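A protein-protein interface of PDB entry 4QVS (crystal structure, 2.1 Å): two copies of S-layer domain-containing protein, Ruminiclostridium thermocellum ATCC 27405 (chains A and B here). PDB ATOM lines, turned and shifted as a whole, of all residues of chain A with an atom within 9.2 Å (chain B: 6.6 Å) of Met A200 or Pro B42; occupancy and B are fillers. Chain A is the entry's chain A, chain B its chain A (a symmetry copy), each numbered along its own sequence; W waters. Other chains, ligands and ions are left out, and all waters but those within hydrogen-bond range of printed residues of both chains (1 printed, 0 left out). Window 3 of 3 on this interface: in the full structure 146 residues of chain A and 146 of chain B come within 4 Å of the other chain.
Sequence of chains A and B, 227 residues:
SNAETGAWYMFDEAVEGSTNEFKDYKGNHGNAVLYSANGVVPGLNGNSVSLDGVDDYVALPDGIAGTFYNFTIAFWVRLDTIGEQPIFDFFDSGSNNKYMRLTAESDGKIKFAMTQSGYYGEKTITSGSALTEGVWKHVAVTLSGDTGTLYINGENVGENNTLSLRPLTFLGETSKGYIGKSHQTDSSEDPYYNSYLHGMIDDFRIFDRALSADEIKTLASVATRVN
Met A200 touches six residues of chain B.
Pro B42 touches one residue of chain A.
Val B41 touches one residue of chain A.
No residue of chain A comes within 4 Å of Gly B43.
Of the printed residues of chain B, Ile A201 touches Ser B48, Val B49, Trp B76 and Val B77.
Of the printed residues of chain A, Leu B44 touches Trp A136 (3.7 Å) and Asp A202 (3.9 Å).
Of the printed residues of chain B, Trp A136 touches Leu B44, Ser B48, Trp B76, Val B77 and Arg B78.
Printed residues of chain A within 4 Å of Arg B78: Gly A134, Val A135, Trp A136, Gly A199 and Met A200.
Gly B46 touches none of the printed residues of chain A.
The nearest residue of chain B that does not touch Met A200 is Trp B76 (4.2 Å).
The nearest residue of chain A that does not touch Pro B42 is Trp A136 (6.0 Å).
The nearest printed residue of chain A that does not touch Val B77 is Leu A131 (4.2 Å).
Water W1 lies within hydrogen-bond range of the backbone carbonyl oxygen (O) of Val A135 (2.5 Å) and the backbone NH (N) of Leu B79 (2.7 Å).
The backbone NH of Gly A134 is in hydrogen-bond range of the backbone carbonyl oxygen of Leu B79 (2.9 Å).
O of Val B77 lies within hydrogen-bond range of N of Lys A137, at 2.8 Å.
The backbone carbonyl oxygen of Phe B75 sits at hydrogen-bond distance from the backbone NH of Val A139 (2.7 Å).
N of Asp B80 sits at hydrogen-bond distance from O of His A198 (2.8 Å).
The backbone carbonyl oxygen (O) of Gly A199 sits at hydrogen-bond distance from the backbone NH (N) of Leu B51 (2.9 Å).
N of Arg B78 lies within hydrogen-bond range of O of Met A200.
The backbone NH (N) of Ile A201 is in hydrogen-bond range of the backbone carbonyl oxygen (O) of Val B49, at 3.1 Å.
The side-chain carboxylate (OD2) of Asp A202 is in hydrogen-bond range of the side-chain hydroxyl (OG) of Ser B48 (2.6 Å).
O of Trp B76 is in hydrogen-bond range of N of Asp A202, 3.0 Å away.
The backbone carbonyl oxygen (O) of Asn B47 lies close to the side-chain carboxylate (OD2) of Asp A202.
Among the printed residues, merely in contact across the chains: Gly A199 with Arg B78 (3.1 Å), Met A200 with Val B41 (3.1 Å), Met A200 with Val B49 (3.1 Å), Lys A137 with Trp B76 (3.2 Å), Leu A197 with Leu B51 (3.3 Å), Ile A201 with Trp B76 (3.4 Å), Met A200 with Val B77 (3.4 Å), Leu A197 with Leu B79 (3.4 Å), Trp A136 with Val B77 (3.4 Å), Met A200 with Pro B42 (3.5 Å), Gly A134 with Arg B78 (3.5 Å), Asp A203 with Phe B75 (3.5 Å), His A198 with Leu B51 (3.5 Å), Trp A136 with Arg B78 (3.6 Å), Phe A204 with Phe B75 (3.6 Å), Val A139 with Val B77 (3.6 Å), Ile A201 with Ser B48 (3.7 Å), Gly A199 with Asp B80 (3.7 Å), Gly A199 with Ser B50 (3.7 Å), Trp A136 with Leu B44 (3.7 Å), Val A135 with Arg B78 (3.7 Å), His A198 with Leu B79 (3.7 Å), Ile A201 with Val B77 (3.8 Å), Trp A136 with Ser B48 (3.8 Å), Asp A202 with Phe B75 (3.8 Å), Trp A136 with Trp B76 (3.8 Å), Val A135 with Val B77 (3.8 Å), Asp A202 with Leu B44 (3.9 Å), Gly A134 with Asp B80 (3.9 Å), Met A200 with Ser B50 (3.96 Å) and Gly A199 with Val B49 (3.99 Å).
The backbone carbonyl oxygen (O) of Val B41 lies close to the side-chain amide oxygen (OD1) of Asn B47.
The backbone carbonyl oxygen (O) of Val B41 sits at hydrogen-bond distance from the backbone NH (N) of Ser B48, 2.9 Å away.
N of Leu B44 lies within hydrogen-bond range of OG of Ser B48.
The side-chain carboxylate (OD1) of Asp B80 lies within salt-bridge range of the guanidinium group (NH1) of Arg B78, 2.7 Å away.
Of the 15 printed residues of chain A, 13 touch a printed residue of chain B.
Printed residues of chain A that touch a printed residue of chain B: Gly A134, Val A135, Trp A136, Lys A137, Val A139, Leu A197, His A198, Gly A199, Met A200, Ile A201, Asp A202, Asp A203 and Phe A204.
Hydrophobic or aromatic side chains of chain A within 4 Å of the printed part of chain B: Trp A136, Val A139, Leu A197, His A198, Met A200, Ile A201 and Phe A204.
Of the 17 printed residues of chain B, 14 touch a printed residue of chain A.
Hydrophobic or aromatic side chains of chain B within 4 Å of the printed part of chain A: Val B41, Leu B44, Val B49, Leu B51, Phe B75, Trp B76, Val B77 and Leu B79.
Among the printed residues, 41 pairs touch across the chains.
Among the printed residues, no Asp or Glu carboxylate lies within 4 Å of a Lys or Arg side-chain nitrogen of the other chain.
No position is printed for both chains.
Of the 41 pairs that touch across the chains among the printed residues, none has its exchanged pair printed and touching as well.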
ATOM      1  N   LEU A 131     -16.181   3.941 -10.669  1.00  0.00           N
ATOM      2  CA  LEU A 131     -17.328   4.869 -10.522  1.00  0.00           C
ATOM      3  C   LEU A 131     -17.706   5.500 -11.831  1.00  0.00           C
ATOM      4  O   LEU A 131     -16.901   6.206 -12.423  1.00  0.00           O
ATOM      5  CB  LEU A 131     -17.034   6.017  -9.547  1.00  0.00           C
ATOM      6  CG  LEU A 131     -17.045   5.727  -8.075  1.00  0.00           C
ATOM      7  CD1 LEU A 131     -16.658   7.023  -7.309  1.00  0.00           C
ATOM      8  CD2 LEU A 131     -18.429   5.239  -7.676  1.00  0.00           C
ATOM      9  N   GLY A 134     -22.814   9.904 -13.217  1.00  0.00           N
ATOM     10  CA  GLY A 134     -24.257   9.929 -13.013  1.00  0.00           C
ATOM     11  C   GLY A 134     -24.898   8.656 -12.474  1.00  0.00           C
ATOM     12  O   GLY A 134     -26.132   8.556 -12.458  1.00  0.00           O
ATOM     13  N   VAL A 135     -24.090   7.707 -11.993  1.00  0.00           N
ATOM     14  CA  VAL A 135     -24.614   6.452 -11.455  1.00  0.00           C
ATOM     15  C   VAL A 135     -24.306   6.237  -9.964  1.00  0.00           C
ATOM     16  O   VAL A 135     -23.156   6.052  -9.600  1.00  0.00           O
ATOM     17  CB  VAL A 135     -24.052   5.242 -12.237  1.00  0.00           C
ATOM     18  CG1 VAL A 135     -24.546   3.943 -11.623  1.00  0.00           C
ATOM     19  CG2 VAL A 135     -24.418   5.329 -13.716  1.00  0.00           C
ATOM     20  N   TRP A 136     -25.346   6.203  -9.125  1.00  0.00           N
ATOM     21  CA  TRP A 136     -25.199   5.938  -7.677  1.00  0.00           C
ATOM     22  C   TRP A 136     -24.447   4.650  -7.394  1.00  0.00           C
ATOM     23  O   TRP A 136     -24.828   3.604  -7.888  1.00  0.00           O
ATOM     24  CB  TRP A 136     -26.582   5.820  -6.991  1.00  0.00           C
ATOM     25  CG  TRP A 136     -27.238   7.124  -6.650  1.00  0.00           C
ATOM     26  CD1 TRP A 136     -28.296   7.710  -7.281  1.00  0.00           C
ATOM     27  CD2 TRP A 136     -26.861   8.006  -5.587  1.00  0.00           C
ATOM     28  NE1 TRP A 136     -28.611   8.902  -6.663  1.00  0.00           N
ATOM     29  CE2 TRP A 136     -27.744   9.102  -5.617  1.00  0.00           C
ATOM     30  CE3 TRP A 136     -25.877   7.960  -4.604  1.00  0.00           C
ATOM     31  CZ2 TRP A 136     -27.663  10.162  -4.692  1.00  0.00           C
ATOM     32  CZ3 TRP A 136     -25.799   9.016  -3.680  1.00  0.00           C
ATOM     33  CH2 TRP A 136     -26.690  10.091  -3.735  1.00  0.00           C
ATOM     34  N   LYS A 137     -23.382   4.705  -6.610  1.00  0.00           N
ATOM     35  CA  LYS A 137     -22.673   3.478  -6.230  1.00  0.00           C
ATOM     36  C   LYS A 137     -22.329   3.535  -4.734  1.00  0.00           C
ATOM     37  O   LYS A 137     -22.300   4.612  -4.160  1.00  0.00           O
ATOM     38  CB  LYS A 137     -21.418   3.277  -7.097  1.00  0.00           C
ATOM     39  CG  LYS A 137     -21.699   2.802  -8.531  1.00  0.00           C
ATOM     40  CD  LYS A 137     -20.421   2.354  -9.244  1.00  0.00           C
ATOM     41  CE  LYS A 137     -20.687   1.469 -10.474  1.00  0.00           C
ATOM     42  NZ  LYS A 137     -21.290   2.275 -11.556  1.00  0.00           N
ATOM     43  N   VAL A 139     -19.597   3.007  -1.791  1.00  0.00           N
ATOM     44  CA  VAL A 139     -18.168   2.881  -1.615  1.00  0.00           C
ATOM     45  C   VAL A 139     -17.815   2.663  -0.155  1.00  0.00           C
ATOM     46  O   VAL A 139     -18.420   3.251   0.717  1.00  0.00           O
ATOM     47  CB  VAL A 139     -17.439   4.121  -2.137  1.00  0.00           C
ATOM     48  CG1 VAL A 139     -15.940   3.993  -1.908  1.00  0.00           C
ATOM     49  CG2 VAL A 139     -17.722   4.338  -3.620  1.00  0.00           C
ATOM     50  N   ILE A 179     -16.163  16.140   3.640  1.00  0.00           N
ATOM     51  CA  ILE A 179     -16.618  15.315   2.550  1.00  0.00           C
ATOM     52  C   ILE A 179     -16.592  16.282   1.397  1.00  0.00           C
ATOM     53  O   ILE A 179     -17.275  17.292   1.434  1.00  0.00           O
ATOM     54  CB  ILE A 179     -18.065  14.794   2.714  1.00  0.00           C
ATOM     55  CG1 ILE A 179     -18.168  13.853   3.895  1.00  0.00           C
ATOM     56  CG2 ILE A 179     -18.509  14.054   1.471  1.00  0.00           C
ATOM     57  CD1 ILE A 179     -19.585  13.407   4.227  1.00  0.00           C
ATOM     58  N   LEU A 197     -15.558  18.077  -4.988  1.00  0.00           N
ATOM     59  CA  LEU A 197     -16.377  17.017  -5.519  1.00  0.00           C
ATOM     60  C   LEU A 197     -17.670  17.516  -6.147  1.00  0.00           C
ATOM     61  O   LEU A 197     -18.419  18.316  -5.563  1.00  0.00           O
ATOM     62  CB  LEU A 197     -16.702  15.989  -4.431  1.00  0.00           C
ATOM     63  CG  LEU A 197     -17.409  14.700  -4.886  1.00  0.00           C
ATOM     64  CD1 LEU A 197     -16.535  13.934  -5.875  1.00  0.00           C
ATOM     65  CD2 LEU A 197     -17.741  13.844  -3.675  1.00  0.00           C
ATOM     66  N   HIS A 198     -17.898  17.045  -7.375  1.00  0.00           N
ATOM     67  CA  HIS A 198     -19.117  17.273  -8.114  1.00  0.00           C
ATOM     68  C   HIS A 198     -19.942  15.971  -8.071  1.00  0.00           C
ATOM     69  O   HIS A 198     -19.617  14.962  -8.736  1.00  0.00           O
ATOM     70  CB  HIS A 198     -18.808  17.705  -9.537  1.00  0.00           C
ATOM     71  CG  HIS A 198     -20.021  18.058 -10.321  1.00  0.00           C
ATOM     72  ND1 HIS A 198     -20.100  17.892 -11.687  1.00  0.00           N
ATOM     73  CD2 HIS A 198     -21.244  18.480  -9.920  1.00  0.00           C
ATOM     74  CE1 HIS A 198     -21.297  18.271 -12.102  1.00  0.00           C
ATOM     75  NE2 HIS A 198     -22.017  18.610 -11.047  1.00  0.00           N
ATOM     76  N   GLY A 199     -20.978  15.980  -7.237  1.00  0.00           N
ATOM     77  CA  GLY A 199     -21.826  14.809  -7.099  1.00  0.00           C
ATOM     78  C   GLY A 199     -22.753  14.843  -5.921  1.00  0.00           C
ATOM     79  O   GLY A 199     -22.940  15.893  -5.282  1.00  0.00           O
ATOM     80  N   MET A 200     -23.331  13.672  -5.637  1.00  0.00           N
ATOM     81  CA  MET A 200     -24.235  13.500  -4.521  1.00  0.00           C
ATOM     82  C   MET A 200     -23.671  12.481  -3.576  1.00  0.00           C
ATOM     83  O   MET A 200     -22.845  11.638  -3.974  1.00  0.00           O
ATOM     84  CB  MET A 200     -25.619  13.104  -5.023  1.00  0.00           C
ATOM     85  CG  MET A 200     -26.272  14.155  -5.923  1.00  0.00           C
ATOM     86  SD  MET A 200     -28.085  13.473  -6.301  1.00  0.00           S
ATOM     87  CE  MET A 200     -29.288  14.847  -5.648  1.00  0.00           C
ATOM     88  N   ILE A 201     -24.076  12.570  -2.301  1.00  0.00           N
ATOM     89  CA  ILE A 201     -23.590  11.668  -1.245  1.00  0.00           C
ATOM     90  C   ILE A 201     -24.722  11.355  -0.311  1.00  0.00           C
ATOM     91  O   ILE A 201     -25.510  12.241  -0.007  1.00  0.00           O
ATOM     92  CB  ILE A 201     -22.502  12.339  -0.368  1.00  0.00           C
ATOM     93  CG1 ILE A 201     -21.250  12.634  -1.197  1.00  0.00           C
ATOM     94  CG2 ILE A 201     -22.147  11.457   0.852  1.00  0.00           C
ATOM     95  CD1 ILE A 201     -20.339  11.457  -1.446  1.00  0.00           C
ATOM     96  N   ASP A 202     -24.776  10.126   0.195  1.00  0.00           N
ATOM     97  CA  ASP A 202     -25.847   9.768   1.133  1.00  0.00           C
ATOM     98  C   ASP A 202     -25.318   8.708   2.080  1.00  0.00           C
ATOM     99  O   ASP A 202     -24.350   8.035   1.784  1.00  0.00           O
ATOM    100  CB  ASP A 202     -27.086   9.270   0.361  1.00  0.00           C
ATOM    101  CG  ASP A 202     -28.427   9.539   1.089  1.00  0.00           C
ATOM    102  OD1 ASP A 202     -28.490   9.701   2.333  1.00  0.00           O
ATOM    103  OD2 ASP A 202     -29.467   9.581   0.390  1.00  0.00           O
ATOM    104  N   ASP A 203     -26.011   8.560   3.200  1.00  0.00           N
ATOM    105  CA  ASP A 203     -25.709   7.565   4.220  1.00  0.00           C
ATOM    106  C   ASP A 203     -24.246   7.442   4.496  1.00  0.00           C
ATOM    107  O   ASP A 203     -23.685   6.362   4.344  1.00  0.00           O
ATOM    108  CB  ASP A 203     -26.357   6.192   3.861  1.00  0.00           C
ATOM    109  CG  ASP A 203     -27.856   6.235   3.906  1.00  0.00           C
ATOM    110  OD1 ASP A 203     -28.423   6.956   4.741  1.00  0.00           O
ATOM    111  OD2 ASP A 203     -28.498   5.515   3.110  1.00  0.00           O
ATOM    112  N   PHE A 204     -23.616   8.551   4.958  1.00  0.00           N
ATOM    113  CA  PHE A 204     -22.209   8.511   5.258  1.00  0.00           C
ATOM    114  C   PHE A 204     -22.080   7.875   6.634  1.00  0.00           C
ATOM    115  O   PHE A 204     -22.651   8.348   7.617  1.00  0.00           O
ATOM    116  CB  PHE A 204     -21.608   9.901   5.231  1.00  0.00           C
ATOM    117  CG  PHE A 204     -20.125   9.903   5.195  1.00  0.00           C
ATOM    118  CD1 PHE A 204     -19.397   9.882   6.360  1.00  0.00           C
ATOM    119  CD2 PHE A 204     -19.455   9.967   3.986  1.00  0.00           C
ATOM    120  CE1 PHE A 204     -18.014   9.913   6.323  1.00  0.00           C
ATOM    121  CE2 PHE A 204     -18.079  10.013   3.936  1.00  0.00           C
ATOM    122  CZ  PHE A 204     -17.352   9.979   5.109  1.00  0.00           C
ATOM    123  N   VAL B  40     -30.231  19.985   0.687  1.00  0.00           N
ATOM    124  CA  VAL B  40     -30.401  18.548   0.403  1.00  0.00           C
ATOM    125  C   VAL B  40     -31.553  18.388  -0.585  1.00  0.00           C
ATOM    126  O   VAL B  40     -32.468  19.199  -0.597  1.00  0.00           O
ATOM    127  CB  VAL B  40     -30.599  17.660   1.656  1.00  0.00           C
ATOM    128  CG1 VAL B  40     -29.334  17.675   2.502  1.00  0.00           C
ATOM    129  CG2 VAL B  40     -31.823  18.061   2.476  1.00  0.00           C
ATOM    130  N   VAL B  41     -31.507  17.359  -1.410  1.00  0.00           N
ATOM    131  CA  VAL B  41     -32.548  17.186  -2.444  1.00  0.00           C
ATOM    132  C   VAL B  41     -32.885  15.709  -2.632  1.00  0.00           C
ATOM    133  O   VAL B  41     -32.116  14.860  -2.158  1.00  0.00           O
ATOM    134  CB  VAL B  41     -32.072  17.802  -3.778  1.00  0.00           C
ATOM    135  CG1 VAL B  41     -31.806  19.313  -3.658  1.00  0.00           C
ATOM    136  CG2 VAL B  41     -30.819  17.108  -4.269  1.00  0.00           C
ATOM    137  N   PRO B  42     -34.034  15.386  -3.313  1.00  0.00           N
ATOM    138  CA  PRO B  42     -34.350  13.971  -3.482  1.00  0.00           C
ATOM    139  C   PRO B  42     -33.139  13.218  -3.983  1.00  0.00           C
ATOM    140  O   PRO B  42     -32.505  13.677  -4.923  1.00  0.00           O
ATOM    141  CB  PRO B  42     -35.467  13.985  -4.553  1.00  0.00           C
ATOM    142  CG  PRO B  42     -36.186  15.277  -4.300  1.00  0.00           C
ATOM    143  CD  PRO B  42     -35.200  16.233  -3.630  1.00  0.00           C
ATOM    144  N   GLY B  43     -32.791  12.107  -3.345  1.00  0.00           N
ATOM    145  CA  GLY B  43     -31.665  11.296  -3.813  1.00  0.00           C
ATOM    146  C   GLY B  43     -31.899   9.801  -3.672  1.00  0.00           C
ATOM    147  O   GLY B  43     -32.983   9.284  -3.994  1.00  0.00           O
ATOM    148  N   LEU B  44     -30.887   9.092  -3.182  1.00  0.00           N
ATOM    149  CA  LEU B  44     -30.993   7.634  -3.037  1.00  0.00           C
ATOM    150  C   LEU B  44     -31.961   7.206  -1.924  1.00  0.00           C
ATOM    151  O   LEU B  44     -32.900   6.458  -2.198  1.00  0.00           O
ATOM    152  CB  LEU B  44     -29.621   7.006  -2.790  1.00  0.00           C
ATOM    153  CG  LEU B  44     -29.603   5.479  -2.839  1.00  0.00           C
ATOM    154  CD1 LEU B  44     -29.579   4.971  -4.274  1.00  0.00           C
ATOM    155  CD2 LEU B  44     -28.403   4.964  -2.088  1.00  0.00           C
ATOM    156  N   GLY B  46     -34.312   8.943   0.608  1.00  0.00           N
ATOM    157  CA  GLY B  46     -34.980  10.151   1.052  1.00  0.00           C
ATOM    158  C   GLY B  46     -34.273  11.286   0.355  1.00  0.00           C
ATOM    159  O   GLY B  46     -34.389  11.471  -0.858  1.00  0.00           O
ATOM    160  N   ASN B  47     -33.527  12.054   1.124  1.00  0.00           N
ATOM    161  CA  ASN B  47     -32.738  13.124   0.558  1.00  0.00           C
ATOM    162  C   ASN B  47     -31.272  12.802   0.685  1.00  0.00           C
ATOM    163  O   ASN B  47     -30.870  11.907   1.469  1.00  0.00           O
ATOM    164  CB  ASN B  47     -33.079  14.468   1.185  1.00  0.00           C
ATOM    165  CG  ASN B  47     -34.396  15.026   0.668  1.00  0.00           C
ATOM    166  OD1 ASN B  47     -34.635  15.072  -0.534  1.00  0.00           O
ATOM    167  ND2 ASN B  47     -35.236  15.495   1.576  1.00  0.00           N
ATOM    168  N   SER B  48     -30.512  13.536  -0.124  1.00  0.00           N
ATOM    169  CA  SER B  48     -29.076  13.392  -0.293  1.00  0.00           C
ATOM    170  C   SER B  48     -28.411  14.771  -0.501  1.00  0.00           C
ATOM    171  O   SER B  48     -29.015  15.713  -1.025  1.00  0.00           O
ATOM    172  CB  SER B  48     -28.809  12.533  -1.559  1.00  0.00           C
ATOM    173  OG  SER B  48     -29.576  11.326  -1.577  1.00  0.00           O
ATOM    174  N   VAL B  49     -27.155  14.886  -0.081  1.00  0.00           N
ATOM    175  CA  VAL B  49     -26.374  16.109  -0.326  1.00  0.00           C
ATOM    176  C   VAL B  49     -26.027  16.214  -1.805  1.00  0.00           C
ATOM    177  O   VAL B  49     -25.626  15.223  -2.403  1.00  0.00           O
ATOM    178  CB  VAL B  49     -25.043  16.071   0.474  1.00  0.00           C
ATOM    179  CG1 VAL B  49     -24.011  17.043  -0.071  1.00  0.00           C
ATOM    180  CG2 VAL B  49     -25.319  16.325   1.936  1.00  0.00           C
ATOM    181  N   SER B  50     -26.183  17.413  -2.376  1.00  0.00           N
ATOM    182  CA  SER B  50     -25.767  17.687  -3.739  1.00  0.00           C
ATOM    183  C   SER B  50     -24.722  18.820  -3.761  1.00  0.00           C
ATOM    184  O   SER B  50     -25.076  19.981  -3.510  1.00  0.00           O
ATOM    185  CB  SER B  50     -26.938  18.117  -4.584  1.00  0.00           C
ATOM    186  OG  SER B  50     -26.517  18.109  -5.921  1.00  0.00           O
ATOM    187  N   LEU B  51     -23.484  18.468  -4.147  1.00  0.00           N
ATOM    188  CA  LEU B  51     -22.332  19.391  -4.183  1.00  0.00           C
ATOM    189  C   LEU B  51     -22.086  19.860  -5.605  1.00  0.00           C
ATOM    190  O   LEU B  51     -22.044  19.030  -6.531  1.00  0.00           O
ATOM    191  CB  LEU B  51     -21.086  18.669  -3.658  1.00  0.00           C
ATOM    192  CG  LEU B  51     -21.211  17.970  -2.290  1.00  0.00           C
ATOM    193  CD1 LEU B  51     -19.909  17.280  -1.896  1.00  0.00           C
ATOM    194  CD2 LEU B  51     -21.620  18.945  -1.187  1.00  0.00           C
ATOM    195  N   PHE B  75     -20.177   4.870   2.335  1.00  0.00           N
ATOM    196  CA  PHE B  75     -21.200   5.774   1.934  1.00  0.00           C
ATOM    197  C   PHE B  75     -21.629   5.479   0.528  1.00  0.00           C
ATOM    198  O   PHE B  75     -20.952   4.806  -0.216  1.00  0.00           O
ATOM    199  CB  PHE B  75     -20.633   7.191   1.960  1.00  0.00           C
ATOM    200  CG  PHE B  75     -19.378   7.321   1.146  1.00  0.00           C
ATOM    201  CD1 PHE B  75     -18.151   6.942   1.680  1.00  0.00           C
ATOM    202  CD2 PHE B  75     -19.433   7.753  -0.176  1.00  0.00           C
ATOM    203  CE1 PHE B  75     -16.999   7.028   0.924  1.00  0.00           C
ATOM    204  CE2 PHE B  75     -18.286   7.825  -0.939  1.00  0.00           C
ATOM    205  CZ  PHE B  75     -17.075   7.460  -0.393  1.00  0.00           C
ATOM    206  N   TRP B  76     -22.722   6.097   0.150  1.00  0.00           N
ATOM    207  CA  TRP B  76     -23.180   6.043  -1.223  1.00  0.00           C
ATOM    208  C   TRP B  76     -22.761   7.325  -1.901  1.00  0.00           C
ATOM    209  O   TRP B  76     -22.854   8.395  -1.288  1.00  0.00           O
ATOM    210  CB  TRP B  76     -24.696   6.006  -1.244  1.00  0.00           C
ATOM    211  CG  TRP B  76     -25.248   4.691  -0.993  1.00  0.00           C
ATOM    212  CD1 TRP B  76     -25.671   4.163   0.195  1.00  0.00           C
ATOM    213  CD2 TRP B  76     -25.505   3.692  -2.008  1.00  0.00           C
ATOM    214  NE1 TRP B  76     -26.170   2.865  -0.022  1.00  0.00           N
ATOM    215  CE2 TRP B  76     -26.073   2.566  -1.361  1.00  0.00           C
ATOM    216  CE3 TRP B  76     -25.292   3.648  -3.388  1.00  0.00           C
ATOM    217  CZ2 TRP B  76     -26.439   1.382  -2.070  1.00  0.00           C
ATOM    218  CZ3 TRP B  76     -25.657   2.460  -4.105  1.00  0.00           C
ATOM    219  CH2 TRP B  76     -26.226   1.354  -3.431  1.00  0.00           C
ATOM    220  N   VAL B  77     -22.372   7.227  -3.164  1.00  0.00           N
ATOM    221  CA  VAL B  77     -22.030   8.372  -3.953  1.00  0.00           C
ATOM    222  C   VAL B  77     -22.486   8.328  -5.409  1.00  0.00           C
ATOM    223  O   VAL B  77     -22.498   7.264  -6.006  1.00  0.00           O
ATOM    224  CB  VAL B  77     -20.499   8.592  -3.938  1.00  0.00           C
ATOM    225  CG1 VAL B  77     -19.728   7.310  -4.207  1.00  0.00           C
ATOM    226  CG2 VAL B  77     -20.111   9.677  -4.927  1.00  0.00           C
ATOM    227  N   ARG B  78     -22.876   9.487  -5.960  1.00  0.00           N
ATOM    228  CA  ARG B  78     -23.182   9.631  -7.389  1.00  0.00           C
ATOM    229  C   ARG B  78     -22.231  10.691  -7.963  1.00  0.00           C
ATOM    230  O   ARG B  78     -22.435  11.891  -7.782  1.00  0.00           O
ATOM    231  CB  ARG B  78     -24.631  10.036  -7.659  1.00  0.00           C
ATOM    232  CG  ARG B  78     -25.017   9.921  -9.143  1.00  0.00           C
ATOM    233  CD  ARG B  78     -26.486  10.251  -9.413  1.00  0.00           C
ATOM    234  NE  ARG B  78     -26.790  11.663  -9.176  1.00  0.00           N
ATOM    235  CZ  ARG B  78     -26.697  12.641 -10.075  1.00  0.00           C
ATOM    236  NH1 ARG B  78     -26.291  12.390 -11.310  1.00  0.00           N
ATOM    237  NH2 ARG B  78     -26.981  13.898  -9.730  1.00  0.00           N
ATOM    238  N   LEU B  79     -21.202  10.233  -8.667  1.00  0.00           N
ATOM    239  CA  LEU B  79     -20.183  11.096  -9.237  1.00  0.00           C
ATOM    240  C   LEU B  79     -20.583  11.757 -10.551  1.00  0.00           C
ATOM    241  O   LEU B  79     -20.699  11.082 -11.586  1.00  0.00           O
ATOM    242  CB  LEU B  79     -18.935  10.272  -9.426  1.00  0.00           C
ATOM    243  CG  LEU B  79     -17.706  11.074  -9.764  1.00  0.00           C
ATOM    244  CD1 LEU B  79     -17.391  11.971  -8.546  1.00  0.00           C
ATOM    245  CD2 LEU B  79     -16.542  10.163 -10.104  1.00  0.00           C
ATOM    246  N   ASP B  80     -20.769  13.080 -10.515  1.00  0.00           N
ATOM    247  CA  ASP B  80     -21.230  13.831 -11.691  1.00  0.00           C
ATOM    248  C   ASP B  80     -20.141  14.393 -12.585  1.00  0.00           C
ATOM    249  O   ASP B  80     -20.440  14.885 -13.660  1.00  0.00           O
ATOM    250  CB  ASP B  80     -22.193  14.920 -11.263  1.00  0.00           C
ATOM    251  CG  ASP B  80     -23.429  14.359 -10.633  1.00  0.00           C
ATOM    252  OD1 ASP B  80     -23.707  13.150 -10.837  1.00  0.00           O
ATOM    253  OD2 ASP B  80     -24.114  15.122  -9.942  1.00  0.00           O
HETATM  254  O   HOH W   1     -21.200   7.673  -9.657  1.00  0.00           O
